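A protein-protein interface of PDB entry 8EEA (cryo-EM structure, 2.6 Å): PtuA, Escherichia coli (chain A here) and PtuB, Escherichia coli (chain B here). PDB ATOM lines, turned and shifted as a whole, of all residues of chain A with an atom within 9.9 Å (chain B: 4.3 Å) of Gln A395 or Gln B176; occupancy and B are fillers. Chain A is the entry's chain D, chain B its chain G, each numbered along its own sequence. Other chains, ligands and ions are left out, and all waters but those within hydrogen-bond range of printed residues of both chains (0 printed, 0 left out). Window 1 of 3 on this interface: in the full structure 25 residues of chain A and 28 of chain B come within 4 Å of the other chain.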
ATOM      1  N   SER A 353      37.661   0.508  -1.213  1.00  0.00           N
ATOM      2  CA  SER A 353      37.343  -0.912  -1.272  1.00  0.00           C
ATOM      3  C   SER A 353      35.937  -1.143  -0.741  1.00  0.00           C
ATOM      4  O   SER A 353      35.658  -0.769   0.407  1.00  0.00           O
ATOM      5  CB  SER A 353      38.357  -1.714  -0.459  1.00  0.00           C
ATOM      6  OG  SER A 353      38.031  -3.091  -0.453  1.00  0.00           O
ATOM      7  N   PRO A 354      35.022  -1.739  -1.512  1.00  0.00           N
ATOM      8  CA  PRO A 354      33.682  -2.007  -0.963  1.00  0.00           C
ATOM      9  C   PRO A 354      33.694  -2.932   0.239  1.00  0.00           C
ATOM     10  O   PRO A 354      32.802  -2.839   1.093  1.00  0.00           O
ATOM     11  CB  PRO A 354      32.934  -2.632  -2.151  1.00  0.00           C
ATOM     12  CG  PRO A 354      33.993  -3.093  -3.085  1.00  0.00           C
ATOM     13  CD  PRO A 354      35.127  -2.142  -2.924  1.00  0.00           C
ATOM     14  N   LEU A 357      33.994  -0.798   3.204  1.00  0.00           N
ATOM     15  CA  LEU A 357      32.832   0.064   3.393  1.00  0.00           C
ATOM     16  C   LEU A 357      31.611  -0.718   3.854  1.00  0.00           C
ATOM     17  O   LEU A 357      30.672  -0.128   4.400  1.00  0.00           O
ATOM     18  CB  LEU A 357      32.518   0.807   2.097  1.00  0.00           C
ATOM     19  CG  LEU A 357      33.492   1.914   1.698  1.00  0.00           C
ATOM     20  CD1 LEU A 357      33.105   2.499   0.354  1.00  0.00           C
ATOM     21  CD2 LEU A 357      33.546   3.000   2.757  1.00  0.00           C
ATOM     22  N   LEU A 367      31.603  11.107   1.489  1.00  0.00           N
ATOM     23  CA  LEU A 367      31.882  11.092   0.058  1.00  0.00           C
ATOM     24  C   LEU A 367      32.212  12.508  -0.396  1.00  0.00           C
ATOM     25  O   LEU A 367      31.415  13.430  -0.192  1.00  0.00           O
ATOM     26  CB  LEU A 367      30.687  10.543  -0.718  1.00  0.00           C
ATOM     27  CG  LEU A 367      30.301   9.095  -0.416  1.00  0.00           C
ATOM     28  CD1 LEU A 367      28.799   8.917  -0.498  1.00  0.00           C
ATOM     29  CD2 LEU A 367      31.001   8.153  -1.373  1.00  0.00           C
ATOM     30  N   PRO A 381      26.266   8.460   2.480  1.00  0.00           N
ATOM     31  CA  PRO A 381      25.509   7.613   1.550  1.00  0.00           C
ATOM     32  C   PRO A 381      24.012   7.701   1.812  1.00  0.00           C
ATOM     33  O   PRO A 381      23.564   7.841   2.951  1.00  0.00           O
ATOM     34  CB  PRO A 381      26.046   6.205   1.826  1.00  0.00           C
ATOM     35  CG  PRO A 381      27.347   6.402   2.508  1.00  0.00           C
ATOM     36  CD  PRO A 381      27.252   7.689   3.254  1.00  0.00           C
ATOM     37  N   LEU A 382      23.234   7.621   0.730  1.00  0.00           N
ATOM     38  CA  LEU A 382      21.781   7.681   0.849  1.00  0.00           C
ATOM     39  C   LEU A 382      21.188   6.377   1.363  1.00  0.00           C
ATOM     40  O   LEU A 382      20.116   6.393   1.978  1.00  0.00           O
ATOM     41  CB  LEU A 382      21.160   8.031  -0.505  1.00  0.00           C
ATOM     42  CG  LEU A 382      21.218   9.496  -0.944  1.00  0.00           C
ATOM     43  CD1 LEU A 382      20.692   9.642  -2.359  1.00  0.00           C
ATOM     44  CD2 LEU A 382      20.430  10.385   0.003  1.00  0.00           C
ATOM     45  N   GLY A 383      21.855   5.247   1.124  1.00  0.00           N
ATOM     46  CA  GLY A 383      21.368   3.952   1.536  1.00  0.00           C
ATOM     47  C   GLY A 383      22.271   3.300   2.574  1.00  0.00           C
ATOM     48  O   GLY A 383      23.408   3.707   2.804  1.00  0.00           O
ATOM     49  N   ALA A 384      21.732   2.261   3.202  1.00  0.00           N
ATOM     50  CA  ALA A 384      22.455   1.553   4.248  1.00  0.00           C
ATOM     51  C   ALA A 384      23.656   0.810   3.673  1.00  0.00           C
ATOM     52  O   ALA A 384      23.622   0.297   2.553  1.00  0.00           O
ATOM     53  CB  ALA A 384      21.530   0.567   4.961  1.00  0.00           C
ATOM     54  N   THR A 385      24.729   0.761   4.461  1.00  0.00           N
ATOM     55  CA  THR A 385      25.941   0.043   4.082  1.00  0.00           C
ATOM     56  C   THR A 385      26.399  -0.979   5.108  1.00  0.00           C
ATOM     57  O   THR A 385      27.315  -1.752   4.803  1.00  0.00           O
ATOM     58  CB  THR A 385      27.097   1.027   3.836  1.00  0.00           C
ATOM     59  OG1 THR A 385      27.615   1.486   5.089  1.00  0.00           O
ATOM     60  CG2 THR A 385      26.629   2.218   3.019  1.00  0.00           C
ATOM     61  N   GLU A 388      25.772  -5.013   4.375  1.00  0.00           N
ATOM     62  CA  GLU A 388      25.230  -5.264   3.052  1.00  0.00           C
ATOM     63  C   GLU A 388      26.256  -5.969   2.170  1.00  0.00           C
ATOM     64  O   GLU A 388      27.461  -5.895   2.419  1.00  0.00           O
ATOM     65  CB  GLU A 388      24.803  -3.953   2.404  1.00  0.00           C
ATOM     66  CG  GLU A 388      23.887  -3.104   3.269  1.00  0.00           C
ATOM     67  CD  GLU A 388      22.697  -3.877   3.801  1.00  0.00           C
ATOM     68  OE1 GLU A 388      22.173  -4.743   3.070  1.00  0.00           O
ATOM     69  OE2 GLU A 388      22.285  -3.621   4.951  1.00  0.00           O
ATOM     70  N   PRO A 389      25.802  -6.663   1.125  1.00  0.00           N
ATOM     71  CA  PRO A 389      26.745  -7.316   0.212  1.00  0.00           C
ATOM     72  C   PRO A 389      27.644  -6.303  -0.484  1.00  0.00           C
ATOM     73  O   PRO A 389      27.328  -5.118  -0.592  1.00  0.00           O
ATOM     74  CB  PRO A 389      25.837  -8.038  -0.788  1.00  0.00           C
ATOM     75  CG  PRO A 389      24.533  -8.180  -0.094  1.00  0.00           C
ATOM     76  CD  PRO A 389      24.405  -6.990   0.796  1.00  0.00           C
ATOM     77  N   SER A 390      28.787  -6.798  -0.962  1.00  0.00           N
ATOM     78  CA  SER A 390      29.798  -5.916  -1.535  1.00  0.00           C
ATOM     79  C   SER A 390      29.306  -5.245  -2.813  1.00  0.00           C
ATOM     80  O   SER A 390      29.604  -4.071  -3.050  1.00  0.00           O
ATOM     81  CB  SER A 390      31.079  -6.700  -1.806  1.00  0.00           C
ATOM     82  OG  SER A 390      31.702  -7.078  -0.592  1.00  0.00           O
ATOM     83  N   ASN A 391      28.577  -5.973  -3.660  1.00  0.00           N
ATOM     84  CA  ASN A 391      28.096  -5.383  -4.906  1.00  0.00           C
ATOM     85  C   ASN A 391      27.082  -4.277  -4.637  1.00  0.00           C
ATOM     86  O   ASN A 391      27.043  -3.268  -5.356  1.00  0.00           O
ATOM     87  CB  ASN A 391      27.491  -6.460  -5.806  1.00  0.00           C
ATOM     88  CG  ASN A 391      26.389  -7.244  -5.121  1.00  0.00           C
ATOM     89  OD1 ASN A 391      26.220  -7.172  -3.908  1.00  0.00           O
ATOM     90  ND2 ASN A 391      25.626  -7.995  -5.905  1.00  0.00           N
ATOM     91  N   ASP A 392      26.247  -4.452  -3.611  1.00  0.00           N
ATOM     92  CA  ASP A 392      25.299  -3.408  -3.240  1.00  0.00           C
ATOM     93  C   ASP A 392      26.027  -2.121  -2.871  1.00  0.00           C
ATOM     94  O   ASP A 392      25.645  -1.032  -3.308  1.00  0.00           O
ATOM     95  CB  ASP A 392      24.434  -3.882  -2.073  1.00  0.00           C
ATOM     96  CG  ASP A 392      23.189  -4.607  -2.529  1.00  0.00           C
ATOM     97  OD1 ASP A 392      23.187  -5.142  -3.657  1.00  0.00           O
ATOM     98  OD2 ASP A 392      22.209  -4.646  -1.756  1.00  0.00           O
ATOM     99  N   VAL A 393      27.086  -2.232  -2.070  1.00  0.00           N
ATOM    100  CA  VAL A 393      27.857  -1.054  -1.689  1.00  0.00           C
ATOM    101  C   VAL A 393      28.569  -0.472  -2.903  1.00  0.00           C
ATOM    102  O   VAL A 393      28.657   0.752  -3.062  1.00  0.00           O
ATOM    103  CB  VAL A 393      28.848  -1.407  -0.566  1.00  0.00           C
ATOM    104  CG1 VAL A 393      29.718  -0.211  -0.219  1.00  0.00           C
ATOM    105  CG2 VAL A 393      28.104  -1.897   0.661  1.00  0.00           C
ATOM    106  N   LEU A 394      29.089  -1.334  -3.776  1.00  0.00           N
ATOM    107  CA  LEU A 394      29.816  -0.862  -4.947  1.00  0.00           C
ATOM    108  C   LEU A 394      28.923  -0.025  -5.853  1.00  0.00           C
ATOM    109  O   LEU A 394      29.332   1.042  -6.324  1.00  0.00           O
ATOM    110  CB  LEU A 394      30.388  -2.057  -5.712  1.00  0.00           C
ATOM    111  CG  LEU A 394      31.343  -1.759  -6.869  1.00  0.00           C
ATOM    112  CD1 LEU A 394      32.616  -1.103  -6.372  1.00  0.00           C
ATOM    113  CD2 LEU A 394      31.660  -3.035  -7.624  1.00  0.00           C
ATOM    114  N   GLN A 395      27.697  -0.488  -6.107  1.00  0.00           N
ATOM    115  CA  GLN A 395      26.826   0.239  -7.025  1.00  0.00           C
ATOM    116  C   GLN A 395      26.124   1.408  -6.342  1.00  0.00           C
ATOM    117  O   GLN A 395      26.011   2.491  -6.925  1.00  0.00           O
ATOM    118  CB  GLN A 395      25.791  -0.704  -7.638  1.00  0.00           C
ATOM    119  CG  GLN A 395      24.975  -0.056  -8.744  1.00  0.00           C
ATOM    120  CD  GLN A 395      24.066  -1.031  -9.457  1.00  0.00           C
ATOM    121  OE1 GLN A 395      23.674  -2.057  -8.901  1.00  0.00           O
ATOM    122  NE2 GLN A 395      23.725  -0.718 -10.700  1.00  0.00           N
ATOM    123  N   SER A 396      25.649   1.212  -5.111  1.00  0.00           N
ATOM    124  CA  SER A 396      24.857   2.240  -4.449  1.00  0.00           C
ATOM    125  C   SER A 396      25.719   3.414  -4.001  1.00  0.00           C
ATOM    126  O   SER A 396      25.301   4.571  -4.108  1.00  0.00           O
ATOM    127  CB  SER A 396      24.117   1.629  -3.259  1.00  0.00           C
ATOM    128  OG  SER A 396      23.263   2.575  -2.647  1.00  0.00           O
ATOM    129  N   VAL A 397      26.919   3.142  -3.502  1.00  0.00           N
ATOM    130  CA  VAL A 397      27.787   4.173  -2.939  1.00  0.00           C
ATOM    131  C   VAL A 397      28.784   4.690  -3.968  1.00  0.00           C
ATOM    132  O   VAL A 397      28.865   5.893  -4.212  1.00  0.00           O
ATOM    133  CB  VAL A 397      28.514   3.633  -1.686  1.00  0.00           C
ATOM    134  CG1 VAL A 397      29.337   4.732  -1.031  1.00  0.00           C
ATOM    135  CG2 VAL A 397      27.516   3.052  -0.697  1.00  0.00           C
ATOM    136  N   MET A 398      29.554   3.793  -4.579  1.00  0.00           N
ATOM    137  CA  MET A 398      30.615   4.182  -5.497  1.00  0.00           C
ATOM    138  C   MET A 398      30.137   4.338  -6.936  1.00  0.00           C
ATOM    139  O   MET A 398      30.912   4.797  -7.781  1.00  0.00           O
ATOM    140  CB  MET A 398      31.750   3.155  -5.444  1.00  0.00           C
ATOM    141  CG  MET A 398      32.166   2.774  -4.029  1.00  0.00           C
ATOM    142  SD  MET A 398      33.497   1.563  -3.980  1.00  0.00           S
ATOM    143  CE  MET A 398      34.921   2.623  -4.179  1.00  0.00           C
ATOM    144  N   GLY A 399      28.894   3.974  -7.232  1.00  0.00           N
ATOM    145  CA  GLY A 399      28.355   4.167  -8.570  1.00  0.00           C
ATOM    146  C   GLY A 399      29.054   3.370  -9.648  1.00  0.00           C
ATOM    147  O   GLY A 399      29.341   3.908 -10.725  1.00  0.00           O
ATOM    148  N   VAL A 400      29.340   2.097  -9.385  1.00  0.00           N
ATOM    149  CA  VAL A 400      29.978   1.210 -10.351  1.00  0.00           C
ATOM    150  C   VAL A 400      29.102  -0.024 -10.520  1.00  0.00           C
ATOM    151  O   VAL A 400      28.741  -0.675  -9.533  1.00  0.00           O
ATOM    152  CB  VAL A 400      31.399   0.817  -9.908  1.00  0.00           C
ATOM    153  CG1 VAL A 400      31.978  -0.233 -10.843  1.00  0.00           C
ATOM    154  CG2 VAL A 400      32.293   2.039  -9.863  1.00  0.00           C
ATOM    155  N   ASP A 401      28.769  -0.341 -11.762  1.00  0.00           N
ATOM    156  CA  ASP A 401      27.951  -1.514 -12.042  1.00  0.00           C
ATOM    157  C   ASP A 401      28.781  -2.780 -11.846  1.00  0.00           C
ATOM    158  O   ASP A 401      29.862  -2.898 -12.432  1.00  0.00           O
ATOM    159  CB  ASP A 401      27.413  -1.447 -13.469  1.00  0.00           C
ATOM    160  CG  ASP A 401      26.392  -2.526 -13.763  1.00  0.00           C
ATOM    161  OD1 ASP A 401      26.051  -3.296 -12.843  1.00  0.00           O
ATOM    162  OD2 ASP A 401      25.927  -2.605 -14.919  1.00  0.00           O
ATOM    163  N   PRO A 402      28.323  -3.740 -11.035  1.00  0.00           N
ATOM    164  CA  PRO A 402      29.109  -4.975 -10.865  1.00  0.00           C
ATOM    165  C   PRO A 402      29.296  -5.765 -12.148  1.00  0.00           C
ATOM    166  O   PRO A 402      30.235  -6.568 -12.228  1.00  0.00           O
ATOM    167  CB  PRO A 402      28.299  -5.771  -9.828  1.00  0.00           C
ATOM    168  CG  PRO A 402      26.952  -5.139  -9.800  1.00  0.00           C
ATOM    169  CD  PRO A 402      27.166  -3.704 -10.126  1.00  0.00           C
ATOM    170  N   GLN A 403      28.440  -5.574 -13.144  1.00  0.00           N
ATOM    171  CA  GLN A 403      28.583  -6.280 -14.411  1.00  0.00           C
ATOM    172  C   GLN A 403      29.660  -5.602 -15.251  1.00  0.00           C
ATOM    173  O   GLN A 403      29.500  -4.429 -15.609  1.00  0.00           O
ATOM    174  CB  GLN A 403      27.250  -6.291 -15.155  1.00  0.00           C
ATOM    175  CG  GLN A 403      27.302  -6.793 -16.593  1.00  0.00           C
ATOM    176  CD  GLN A 403      27.766  -8.231 -16.704  1.00  0.00           C
ATOM    177  OE1 GLN A 403      28.628  -8.553 -17.521  1.00  0.00           O
ATOM    178  NE2 GLN A 403      27.191  -9.105 -15.887  1.00  0.00           N
ATOM    179  N   LYS A 409      28.016  -7.128 -23.193  1.00  0.00           N
ATOM    180  CA  LYS A 409      27.159  -6.456 -22.221  1.00  0.00           C
ATOM    181  C   LYS A 409      25.957  -5.798 -22.889  1.00  0.00           C
ATOM    182  O   LYS A 409      24.828  -5.910 -22.396  1.00  0.00           O
ATOM    183  CB  LYS A 409      27.962  -5.421 -21.435  1.00  0.00           C
ATOM    184  CG  LYS A 409      27.190  -4.825 -20.270  1.00  0.00           C
ATOM    185  CD  LYS A 409      28.045  -3.901 -19.430  1.00  0.00           C
ATOM    186  CE  LYS A 409      27.234  -3.274 -18.310  1.00  0.00           C
ATOM    187  NZ  LYS A 409      28.043  -2.329 -17.497  1.00  0.00           N
ATOM    188  N   GLN A 413      21.972  -6.418 -22.169  1.00  0.00           N
ATOM    189  CA  GLN A 413      20.998  -5.403 -21.780  1.00  0.00           C
ATOM    190  C   GLN A 413      19.808  -5.393 -22.731  1.00  0.00           C
ATOM    191  O   GLN A 413      18.654  -5.285 -22.294  1.00  0.00           O
ATOM    192  CB  GLN A 413      21.665  -4.028 -21.739  1.00  0.00           C
ATOM    193  CG  GLN A 413      22.842  -3.949 -20.784  1.00  0.00           C
ATOM    194  CD  GLN A 413      23.024  -2.571 -20.191  1.00  0.00           C
ATOM    195  OE1 GLN A 413      22.981  -1.566 -20.900  1.00  0.00           O
ATOM    196  NE2 GLN A 413      23.235  -2.514 -18.882  1.00  0.00           N
ATOM    197  N   GLY B 145      17.146  -3.689 -12.447  1.00  0.00           N
ATOM    198  CA  GLY B 145      17.031  -2.456 -11.701  1.00  0.00           C
ATOM    199  C   GLY B 145      16.920  -1.205 -12.542  1.00  0.00           C
ATOM    200  O   GLY B 145      16.838  -0.109 -11.977  1.00  0.00           O
ATOM    201  N   ARG B 146      16.909  -1.330 -13.865  1.00  0.00           N
ATOM    202  CA  ARG B 146      16.828  -0.166 -14.733  1.00  0.00           C
ATOM    203  C   ARG B 146      15.373   0.204 -15.014  1.00  0.00           C
ATOM    204  O   ARG B 146      14.444  -0.572 -14.784  1.00  0.00           O
ATOM    205  CB  ARG B 146      17.558  -0.428 -16.047  1.00  0.00           C
ATOM    206  CG  ARG B 146      19.034  -0.078 -16.029  1.00  0.00           C
ATOM    207  CD  ARG B 146      19.669  -0.317 -17.389  1.00  0.00           C
ATOM    208  NE  ARG B 146      19.369  -1.651 -17.898  1.00  0.00           N
ATOM    209  CZ  ARG B 146      19.081  -1.939 -19.161  1.00  0.00           C
ATOM    210  NH1 ARG B 146      19.064  -1.006 -20.100  1.00  0.00           N
ATOM    211  NH2 ARG B 146      18.800  -3.195 -19.490  1.00  0.00           N
ATOM    212  N   ASN B 171      18.054   6.659 -13.010  1.00  0.00           N
ATOM    213  CA  ASN B 171      18.843   5.441 -13.147  1.00  0.00           C
ATOM    214  C   ASN B 171      20.146   5.516 -12.354  1.00  0.00           C
ATOM    215  O   ASN B 171      21.163   4.951 -12.763  1.00  0.00           O
ATOM    216  CB  ASN B 171      19.128   5.161 -14.624  1.00  0.00           C
ATOM    217  CG  ASN B 171      18.143   4.184 -15.236  1.00  0.00           C
ATOM    218  OD1 ASN B 171      17.537   3.374 -14.539  1.00  0.00           O
ATOM    219  ND2 ASN B 171      17.977   4.260 -16.548  1.00  0.00           N
ATOM    220  N   SER B 172      20.128   6.203 -11.216  1.00  0.00           N
ATOM    221  CA  SER B 172      21.300   6.256 -10.359  1.00  0.00           C
ATOM    222  C   SER B 172      21.500   4.918  -9.651  1.00  0.00           C
ATOM    223  O   SER B 172      20.594   4.085  -9.566  1.00  0.00           O
ATOM    224  CB  SER B 172      21.165   7.380  -9.332  1.00  0.00           C
ATOM    225  OG  SER B 172      19.971   7.250  -8.584  1.00  0.00           O
ATOM    226  N   GLY B 173      22.714   4.718  -9.135  1.00  0.00           N
ATOM    227  CA  GLY B 173      23.037   3.450  -8.503  1.00  0.00           C
ATOM    228  C   GLY B 173      22.134   3.126  -7.329  1.00  0.00           C
ATOM    229  O   GLY B 173      21.730   1.975  -7.144  1.00  0.00           O
ATOM    230  N   PHE B 174      21.804   4.134  -6.520  1.00  0.00           N
ATOM    231  CA  PHE B 174      20.953   3.905  -5.356  1.00  0.00           C
ATOM    232  C   PHE B 174      19.572   3.405  -5.774  1.00  0.00           C
ATOM    233  O   PHE B 174      19.076   2.394  -5.257  1.00  0.00           O
ATOM    234  CB  PHE B 174      20.856   5.198  -4.543  1.00  0.00           C
ATOM    235  CG  PHE B 174      19.857   5.151  -3.426  1.00  0.00           C
ATOM    236  CD1 PHE B 174      20.042   4.310  -2.347  1.00  0.00           C
ATOM    237  CD2 PHE B 174      18.737   5.962  -3.448  1.00  0.00           C
ATOM    238  CE1 PHE B 174      19.125   4.269  -1.321  1.00  0.00           C
ATOM    239  CE2 PHE B 174      17.818   5.925  -2.422  1.00  0.00           C
ATOM    240  CZ  PHE B 174      18.014   5.078  -1.358  1.00  0.00           C
ATOM    241  N   LEU B 175      18.945   4.095  -6.731  1.00  0.00           N
ATOM    242  CA  LEU B 175      17.622   3.691  -7.193  1.00  0.00           C
ATOM    243  C   LEU B 175      17.666   2.325  -7.864  1.00  0.00           C
ATOM    244  O   LEU B 175      16.760   1.504  -7.681  1.00  0.00           O
ATOM    245  CB  LEU B 175      17.062   4.740  -8.155  1.00  0.00           C
ATOM    246  CG  LEU B 175      16.532   6.033  -7.532  1.00  0.00           C
ATOM    247  CD1 LEU B 175      16.168   7.032  -8.616  1.00  0.00           C
ATOM    248  CD2 LEU B 175      15.339   5.761  -6.636  1.00  0.00           C
ATOM    249  N   GLN B 176      18.708   2.067  -8.656  1.00  0.00           N
ATOM    250  CA  GLN B 176      18.827   0.773  -9.316  1.00  0.00           C
ATOM    251  C   GLN B 176      18.940  -0.354  -8.297  1.00  0.00           C
ATOM    252  O   GLN B 176      18.295  -1.399  -8.441  1.00  0.00           O
ATOM    253  CB  GLN B 176      20.031   0.774 -10.254  1.00  0.00           C
ATOM    254  CG  GLN B 176      19.816   1.572 -11.531  1.00  0.00           C
ATOM    255  CD  GLN B 176      20.864   1.283 -12.583  1.00  0.00           C
ATOM    256  OE1 GLN B 176      21.025   0.146 -13.019  1.00  0.00           O
ATOM    257  NE2 GLN B 176      21.581   2.317 -13.001  1.00  0.00           N
ATOM    258  N   THR B 177      19.749  -0.158  -7.254  1.00  0.00           N
ATOM    259  CA  THR B 177      19.881  -1.181  -6.222  1.00  0.00           C
ATOM    260  C   THR B 177      18.558  -1.416  -5.503  1.00  0.00           C
ATOM    261  O   THR B 177      18.157  -2.567  -5.278  1.00  0.00           O
ATOM    262  CB  THR B 177      20.966  -0.779  -5.224  1.00  0.00           C
ATOM    263  OG1 THR B 177      22.139  -0.361  -5.934  1.00  0.00           O
ATOM    264  CG2 THR B 177      21.317  -1.940  -4.312  1.00  0.00           C
ATOM    265  N   GLU B 178      17.861  -0.338  -5.138  1.00  0.00           N
ATOM    266  CA  GLU B 178      16.587  -0.499  -4.444  1.00  0.00           C
ATOM    267  C   GLU B 178      15.578  -1.246  -5.310  1.00  0.00           C
ATOM    268  O   GLU B 178      14.884  -2.154  -4.832  1.00  0.00           O
ATOM    269  CB  GLU B 178      16.035   0.867  -4.033  1.00  0.00           C
ATOM    270  CG  GLU B 178      16.889   1.633  -3.025  1.00  0.00           C
ATOM    271  CD  GLU B 178      17.412   0.762  -1.897  1.00  0.00           C
ATOM    272  OE1 GLU B 178      16.658  -0.103  -1.408  1.00  0.00           O
ATOM    273  OE2 GLU B 178      18.581   0.944  -1.497  1.00  0.00           O
ATOM    274  N   ARG B 179      15.490  -0.888  -6.594  1.00  0.00           N
ATOM    275  CA  ARG B 179      14.528  -1.536  -7.477  1.00  0.00           C
ATOM    276  C   ARG B 179      14.891  -3.000  -7.715  1.00  0.00           C
ATOM    277  O   ARG B 179      14.006  -3.859  -7.801  1.00  0.00           O
ATOM    278  CB  ARG B 179      14.442  -0.768  -8.795  1.00  0.00           C
ATOM    279  CG  ARG B 179      13.685   0.554  -8.677  1.00  0.00           C
ATOM    280  CD  ARG B 179      13.339   1.147 -10.035  1.00  0.00           C
ATOM    281  NE  ARG B 179      14.527   1.437 -10.831  1.00  0.00           N
ATOM    282  CZ  ARG B 179      14.979   2.652 -11.117  1.00  0.00           C
ATOM    283  NH1 ARG B 179      14.360   3.742 -10.693  1.00  0.00           N
ATOM    284  NH2 ARG B 179      16.080   2.777 -11.848  1.00  0.00           N
ATOM    285  N   ARG B 180      16.188  -3.305  -7.816  1.00  0.00           N
ATOM    286  CA  ARG B 180      16.613  -4.693  -7.962  1.00  0.00           C
ATOM    287  C   ARG B 180      16.225  -5.519  -6.741  1.00  0.00           C
ATOM    288  O   ARG B 180      15.743  -6.653  -6.870  1.00  0.00           O
ATOM    289  CB  ARG B 180      18.121  -4.743  -8.189  1.00  0.00           C
ATOM    290  CG  ARG B 180      18.619  -6.010  -8.848  1.00  0.00           C
ATOM    291  CD  ARG B 180      20.047  -5.835  -9.329  1.00  0.00           C
ATOM    292  NE  ARG B 180      20.924  -5.362  -8.262  1.00  0.00           N
ATOM    293  CZ  ARG B 180      21.673  -4.269  -8.314  1.00  0.00           C
ATOM    294  NH1 ARG B 180      21.683  -3.480  -9.376  1.00  0.00           N
ATOM    295  NH2 ARG B 180      22.439  -3.959  -7.272  1.00  0.00           N
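OD1 of Asp A392 is in salt-bridge range of NH2 of Arg B180, at 3.9 Å.
The guanidinium group (NH1) of Arg B180 is in hydrogen-bond range of the side-chain amide oxygen (OE1) of Gln A395.
The backbone carbonyl oxygen (O) of Asn B171 is in hydrogen-bond range of the side-chain amide nitrogen (NE2) of Gln B176.
O of Gly B173 is in hydrogen-bond range of OG1 of Thr B177 (2.7 Å).
Among the printed residues, pairs that only touch across the chains: Leu A382 with Phe B174, Gly A383 with Phe B174, Asp A392 with Thr B177, Gln A395 with Gly B173, Gln A395 with Gln B176, Gln A395 with Thr B177, Ser A396 with Phe B174, Ser A396 with Thr B177 and Gln A413 with Arg B146.
Ser A353 touches none of the printed residues of chain B.
Printed residues of chain B within 4 Å of Gly A383: Phe B174.
Printed residues of chain B within 4 Å of Asp A392: Thr B177 and Arg B180.
Gln A395 touches four residues of chain B.
Gln A403 touches none of the printed residues of chain B.
Printed residues of chain B within 4 Å of Gln A413: Arg B146 (3.5 Å).
No residue of chain A comes within 4 Å of Gly B145.
No residue of chain A comes within 4 Å of Asn B171.
Of chain A, only Gln A395 (3.5 Å) comes within 4 Å of Gly B173.
No residue of chain A comes within 4 Å of Leu B175.
Gln B176 touches just one residue of chain A: Gln A395.
Thr B177 touches just these residues of chain A: Asp A392, Gln A395 and Ser A396.
No residue of chain A comes within 4 Å of Arg B179.
Of the printed residues of chain A, Arg B180 touches Asp A392 (3.9 Å) and Gln A395 (2.5 Å).
The nearest printed residue of chain B that does not touch Gln A395 is Phe B174 (4.5 Å).
The nearest residue of chain A that does not touch Gln B176 is Asp A401 (5.9 Å).
The nearest printed residue of chain B that does not touch Leu A382 is Glu B178 (6.6 Å).
Printed residues of chain A that touch a printed residue of chain B: Leu A382, Gly A383, Asp A392, Gln A395, Ser A396 and Gln A413.
Of the 12 printed residues of chain B, 6 touch a printed residue of chain A.
Hydrophobic or aromatic side chains of chain B that line the printed part of chain A: Phe B174.
Among the printed residues, Asp or Glu carboxylates within 4 Å of a Lys or Arg side-chain nitrogen of the other chain: Asp A392 with Arg B180.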
